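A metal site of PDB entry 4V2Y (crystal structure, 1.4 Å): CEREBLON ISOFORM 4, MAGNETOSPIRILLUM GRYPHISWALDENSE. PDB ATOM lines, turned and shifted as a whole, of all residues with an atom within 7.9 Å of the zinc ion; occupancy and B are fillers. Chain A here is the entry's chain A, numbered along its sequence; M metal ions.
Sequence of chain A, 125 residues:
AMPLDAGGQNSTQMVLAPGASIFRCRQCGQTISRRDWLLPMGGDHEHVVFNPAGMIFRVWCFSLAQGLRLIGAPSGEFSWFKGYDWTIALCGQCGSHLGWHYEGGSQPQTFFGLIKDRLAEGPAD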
ATOM      1  N   ARG A  24     -23.544   4.169 -33.193  1.00  0.00           N
ATOM      2  CA  ARG A  24     -23.340   4.204 -31.802  1.00  0.00           C
ATOM      3  C   ARG A  24     -22.529   5.448 -31.420  1.00  0.00           C
ATOM      4  O   ARG A  24     -21.762   5.945 -32.228  1.00  0.00           O
ATOM      5  CB  ARG A  24     -22.612   2.936 -31.273  1.00  0.00           C
ATOM      6  CG  ARG A  24     -23.439   1.714 -31.472  1.00  0.00           C
ATOM      7  CD  ARG A  24     -22.816   0.415 -30.889  1.00  0.00           C
ATOM      8  NE  ARG A  24     -23.654  -0.713 -30.967  1.00  0.00           N
ATOM      9  CZ  ARG A  24     -24.732  -0.888 -30.251  1.00  0.00           C
ATOM     10  NH1 ARG A  24     -24.898  -0.139 -29.219  1.00  0.00           N
ATOM     11  NH2 ARG A  24     -25.613  -1.894 -30.452  1.00  0.00           N
ATOM     12  N   CYS A  25     -22.591   5.877 -30.158  1.00  0.00           N
ATOM     13  CA  CYS A  25     -21.672   6.894 -29.627  1.00  0.00           C
ATOM     14  C   CYS A  25     -20.255   6.410 -29.718  1.00  0.00           C
ATOM     15  O   CYS A  25     -19.928   5.331 -29.237  1.00  0.00           O
ATOM     16  CB  CYS A  25     -22.031   7.215 -28.223  1.00  0.00           C
ATOM     17  SG  CYS A  25     -20.869   8.423 -27.495  1.00  0.00           S
ATOM     18  N   ARG A  26     -19.385   7.156 -30.382  1.00  0.00           N
ATOM     19  CA  ARG A  26     -17.999   6.821 -30.470  1.00  0.00           C
ATOM     20  C   ARG A  26     -17.267   6.681 -29.176  1.00  0.00           C
ATOM     21  O   ARG A  26     -16.273   5.948 -29.107  1.00  0.00           O
ATOM     22  CB  ARG A  26     -17.293   7.846 -31.375  1.00  0.00           C
ATOM     23  CG  ARG A  26     -15.814   7.682 -31.603  1.00  0.00           C
ATOM     24  CD  ARG A  26     -15.292   8.708 -32.562  1.00  0.00           C
ATOM     25  NE  ARG A  26     -13.887   8.624 -32.647  1.00  0.00           N
ATOM     26  CZ  ARG A  26     -13.085   9.364 -33.402  1.00  0.00           C
ATOM     27  NH1 ARG A  26     -13.618  10.315 -34.178  1.00  0.00           N
ATOM     28  NH2 ARG A  26     -11.814   9.200 -33.352  1.00  0.00           N
ATOM     29  N   GLN A  27     -17.700   7.442 -28.176  1.00  0.00           N
ATOM     30  CA  GLN A  27     -16.969   7.462 -26.893  1.00  0.00           C
ATOM     31  C   GLN A  27     -17.366   6.379 -25.986  1.00  0.00           C
ATOM     32  O   GLN A  27     -16.554   6.020 -25.094  1.00  0.00           O
ATOM     33  CB  GLN A  27     -17.142   8.779 -26.230  1.00  0.00           C
ATOM     34  CG  GLN A  27     -16.547   9.876 -27.070  1.00  0.00           C
ATOM     35  CD  GLN A  27     -15.100   9.684 -27.498  1.00  0.00           C
ATOM     36  OE1 GLN A  27     -14.718   9.834 -28.680  1.00  0.00           O
ATOM     37  NE2 GLN A  27     -14.304   9.296 -26.581  1.00  0.00           N
ATOM     38  N   CYS A  28     -18.530   5.723 -26.120  1.00  0.00           N
ATOM     39  CA  CYS A  28     -19.019   4.764 -25.180  1.00  0.00           C
ATOM     40  C   CYS A  28     -19.735   3.563 -25.698  1.00  0.00           C
ATOM     41  O   CYS A  28     -19.933   2.607 -24.964  1.00  0.00           O
ATOM     42  CB  CYS A  28     -19.802   5.434 -24.073  1.00  0.00           C
ATOM     43  SG  CYS A  28     -21.483   5.927 -24.541  1.00  0.00           S
ATOM     44  N   GLY A  29     -20.301   3.632 -26.939  1.00  0.00           N
ATOM     45  CA  GLY A  29     -21.050   2.623 -27.479  1.00  0.00           C
ATOM     46  C   GLY A  29     -22.560   2.636 -27.384  1.00  0.00           C
ATOM     47  O   GLY A  29     -23.253   1.776 -27.919  1.00  0.00           O
ATOM     48  N   GLN A  30     -23.119   3.675 -26.722  1.00  0.00           N
ATOM     49  CA  GLN A  30     -24.532   3.822 -26.660  1.00  0.00           C
ATOM     50  C   GLN A  30     -25.200   3.725 -28.035  1.00  0.00           C
ATOM     51  O   GLN A  30     -24.707   4.373 -28.930  1.00  0.00           O
ATOM     52  CB  GLN A  30     -24.834   5.204 -26.067  1.00  0.00           C
ATOM     53  CG  GLN A  30     -26.301   5.558 -26.047  1.00  0.00           C
ATOM     54  CD  GLN A  30     -27.010   5.011 -24.842  1.00  0.00           C
ATOM     55  OE1 GLN A  30     -26.825   3.854 -24.439  1.00  0.00           O
ATOM     56  NE2 GLN A  30     -27.786   5.857 -24.210  1.00  0.00           N
ATOM     57  N   THR A  31     -26.314   2.973 -28.205  1.00  0.00           N
ATOM     58  CA  THR A  31     -27.004   2.957 -29.491  1.00  0.00           C
ATOM     59  C   THR A  31     -27.658   4.325 -29.706  1.00  0.00           C
ATOM     60  O   THR A  31     -28.371   4.801 -28.815  1.00  0.00           O
ATOM     61  CB  THR A  31     -28.101   1.897 -29.442  1.00  0.00           C
ATOM     62  OG1 THR A  31     -27.668   0.711 -28.727  1.00  0.00           O
ATOM     63  CG2 THR A  31     -28.509   1.541 -30.805  1.00  0.00           C
ATOM     64  N   ILE A  32     -27.450   4.913 -30.888  1.00  0.00           N
ATOM     65  CA  ILE A  32     -27.959   6.224 -31.212  1.00  0.00           C
ATOM     66  C   ILE A  32     -28.871   6.262 -32.440  1.00  0.00           C
ATOM     67  O   ILE A  32     -29.979   6.815 -32.351  1.00  0.00           O
ATOM     68  CB  ILE A  32     -26.845   7.268 -31.393  1.00  0.00           C
ATOM     69  CG1 ILE A  32     -25.917   7.375 -30.187  1.00  0.00           C
ATOM     70  CG2 ILE A  32     -27.397   8.638 -31.716  1.00  0.00           C
ATOM     71  CD1 ILE A  32     -26.550   7.874 -28.919  1.00  0.00           C
ATOM     72  N   GLY A  67     -31.303   7.172 -27.320  1.00  0.00           N
ATOM     73  CA  GLY A  67     -30.135   7.084 -26.493  1.00  0.00           C
ATOM     74  C   GLY A  67     -29.505   8.419 -26.183  1.00  0.00           C
ATOM     75  O   GLY A  67     -28.388   8.450 -25.622  1.00  0.00           O
ATOM     76  N   LEU A  90     -27.025  15.432 -26.068  1.00  0.00           N
ATOM     77  CA  LEU A  90     -25.879  14.707 -25.512  1.00  0.00           C
ATOM     78  C   LEU A  90     -26.129  13.209 -25.641  1.00  0.00           C
ATOM     79  O   LEU A  90     -27.290  12.753 -25.569  1.00  0.00           O
ATOM     80  CB  LEU A  90     -25.652  15.044 -24.053  1.00  0.00           C
ATOM     81  CG  LEU A  90     -25.452  16.563 -23.735  1.00  0.00           C
ATOM     82  CD1 LEU A  90     -25.194  16.771 -22.256  1.00  0.00           C
ATOM     83  CD2 LEU A  90     -24.346  17.204 -24.564  1.00  0.00           C
ATOM     84  N   CYS A  91     -25.083  12.411 -25.746  1.00  0.00           N
ATOM     85  CA  CYS A  91     -25.179  10.981 -25.462  1.00  0.00           C
ATOM     86  C   CYS A  91     -25.782  10.855 -24.102  1.00  0.00           C
ATOM     87  O   CYS A  91     -25.293  11.362 -23.086  1.00  0.00           O
ATOM     88  CB  CYS A  91     -23.799  10.370 -25.452  1.00  0.00           C
ATOM     89  SG  CYS A  91     -23.872   8.571 -25.117  1.00  0.00           S
ATOM     90  N   GLY A  92     -26.895  10.082 -23.980  1.00  0.00           N
ATOM     91  CA  GLY A  92     -27.489   9.894 -22.737  1.00  0.00           C
ATOM     92  C   GLY A  92     -26.752   9.053 -21.740  1.00  0.00           C
ATOM     93  O   GLY A  92     -27.063   9.054 -20.530  1.00  0.00           O
ATOM     94  N   GLN A  93     -25.769   8.301 -22.202  1.00  0.00           N
ATOM     95  CA  GLN A  93     -24.934   7.431 -21.348  1.00  0.00           C
ATOM     96  C   GLN A  93     -23.719   8.272 -20.880  1.00  0.00           C
ATOM     97  O   GLN A  93     -23.561   8.443 -19.683  1.00  0.00           O
ATOM     98  CB  GLN A  93     -24.558   6.175 -22.130  1.00  0.00           C
ATOM     99  CG  GLN A  93     -23.703   5.157 -21.341  1.00  0.00           C
ATOM    100  CD  GLN A  93     -23.821   3.765 -21.969  1.00  0.00           C
ATOM    101  OE1 GLN A  93     -24.653   2.966 -21.550  1.00  0.00           O
ATOM    102  NE2 GLN A  93     -23.074   3.548 -23.027  1.00  0.00           N
ATOM    103  N   CYS A  94     -22.888   8.768 -21.812  1.00  0.00           N
ATOM    104  CA  CYS A  94     -21.603   9.372 -21.395  1.00  0.00           C
ATOM    105  C   CYS A  94     -21.575  10.856 -21.448  1.00  0.00           C
ATOM    106  O   CYS A  94     -20.598  11.438 -20.941  1.00  0.00           O
ATOM    107  CB  CYS A  94     -20.456   8.812 -22.210  1.00  0.00           C
ATOM    108  SG  CYS A  94     -20.313   9.520 -23.894  1.00  0.00           S
ATOM    109  N   GLY A  95     -22.570  11.538 -21.980  1.00  0.00           N
ATOM    110  CA  GLY A  95     -22.551  12.995 -21.987  1.00  0.00           C
ATOM    111  C   GLY A  95     -21.816  13.621 -23.128  1.00  0.00           C
ATOM    112  O   GLY A  95     -21.876  14.853 -23.222  1.00  0.00           O
ATOM    113  N   SER A  96     -21.244  12.883 -24.047  1.00  0.00           N
ATOM    114  CA  SER A  96     -20.572  13.436 -25.236  1.00  0.00           C
ATOM    115  C   SER A  96     -21.592  14.277 -26.016  1.00  0.00           C
ATOM    116  O   SER A  96     -22.734  13.875 -26.168  1.00  0.00           O
ATOM    117  CB  SER A  96     -20.085  12.301 -26.102  1.00  0.00           C
ATOM    118  OG  SER A  96     -19.522  12.734 -27.349  1.00  0.00           O
ATOM    119  N   HIS A  97     -21.175  15.424 -26.537  1.00  0.00           N
ATOM    120  CA  HIS A  97     -22.070  16.226 -27.336  1.00  0.00           C
ATOM    121  C   HIS A  97     -22.177  15.660 -28.716  1.00  0.00           C
ATOM    122  O   HIS A  97     -21.236  15.698 -29.547  1.00  0.00           O
ATOM    123  CB  HIS A  97     -21.575  17.646 -27.419  1.00  0.00           C
ATOM    124  CG  HIS A  97     -22.432  18.488 -28.280  1.00  0.00           C
ATOM    125  ND1 HIS A  97     -21.932  19.630 -28.902  1.00  0.00           N
ATOM    126  CD2 HIS A  97     -23.735  18.415 -28.605  1.00  0.00           C
ATOM    127  CE1 HIS A  97     -22.919  20.177 -29.581  1.00  0.00           C
ATOM    128  NE2 HIS A  97     -24.002  19.455 -29.429  1.00  0.00           N
ATOM    129  N   LEU A  98     -23.274  15.001 -29.055  1.00  0.00           N
ATOM    130  CA  LEU A  98     -23.469  14.320 -30.308  1.00  0.00           C
ATOM    131  C   LEU A  98     -24.142  15.137 -31.382  1.00  0.00           C
ATOM    132  O   LEU A  98     -24.058  14.784 -32.550  1.00  0.00           O
ATOM    133  CB  LEU A  98     -24.214  12.983 -30.126  1.00  0.00           C
ATOM    134  CG  LEU A  98     -23.470  11.973 -29.269  1.00  0.00           C
ATOM    135  CD1 LEU A  98     -24.192  10.645 -29.234  1.00  0.00           C
ATOM    136  CD2 LEU A  98     -22.057  11.721 -29.627  1.00  0.00           C
ATOM    137  N   ARG A 118     -18.534  11.947 -34.402  1.00  0.00           N
ATOM    138  CA  ARG A 118     -18.742  11.568 -33.022  1.00  0.00           C
ATOM    139  C   ARG A 118     -19.540  10.258 -32.894  1.00  0.00           C
ATOM    140  O   ARG A 118     -19.886   9.829 -31.791  1.00  0.00           O
ATOM    141  CB  ARG A 118     -19.305  12.746 -32.243  1.00  0.00           C
ATOM    142  CG  ARG A 118     -18.455  14.012 -32.390  1.00  0.00           C
ATOM    143  CD  ARG A 118     -18.965  15.100 -31.422  1.00  0.00           C
ATOM    144  NE  ARG A 118     -18.178  16.287 -31.678  1.00  0.00           N
ATOM    145  CZ  ARG A 118     -18.299  17.431 -31.029  1.00  0.00           C
ATOM    146  NH1 ARG A 118     -19.193  17.598 -30.138  1.00  0.00           N
ATOM    147  NH2 ARG A 118     -17.496  18.435 -31.315  1.00  0.00           N
HETATM  148 ZN    ZN M   1     -21.550   8.130 -25.262  1.00  0.00          ZN
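The side-chain amide nitrogen (NE2) of Gln 93 lies close to the side-chain sulfur (SG) of Cys 28, 3.2 Å away. The side-chain sulfur (SG) of Cys 94 sits close to the backbone NH (N) of Ser 96. SG of Cys 28 lies close to N of Gln 30, 3.5 Å away. N of Gln 27 lies close to SG of Cys 25 (3.4 Å). The backbone NH (N) of Cys 91 is in hydrogen-bond range of the backbone carbonyl oxygen (O) of Ser 96. SG of Cys 91 lies close to N of Gln 93 (3.5 Å). N of Cys 25 sits at hydrogen-bond distance from O of Gln 30 (2.9 Å).
Four residues have an atom within 4 Å of the zinc ion: Cys 25, Cys 28, Cys 91 and Cys 94. The nearest printed residue that does not touch the zinc ion is Gln 30 (4.5 Å).
The zinc ion is bound by SG of Cys 94, SG of Cys 28, SG of Cys 25 and SG of Cys 91. The zinc ion has four donor atoms within binding distance.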
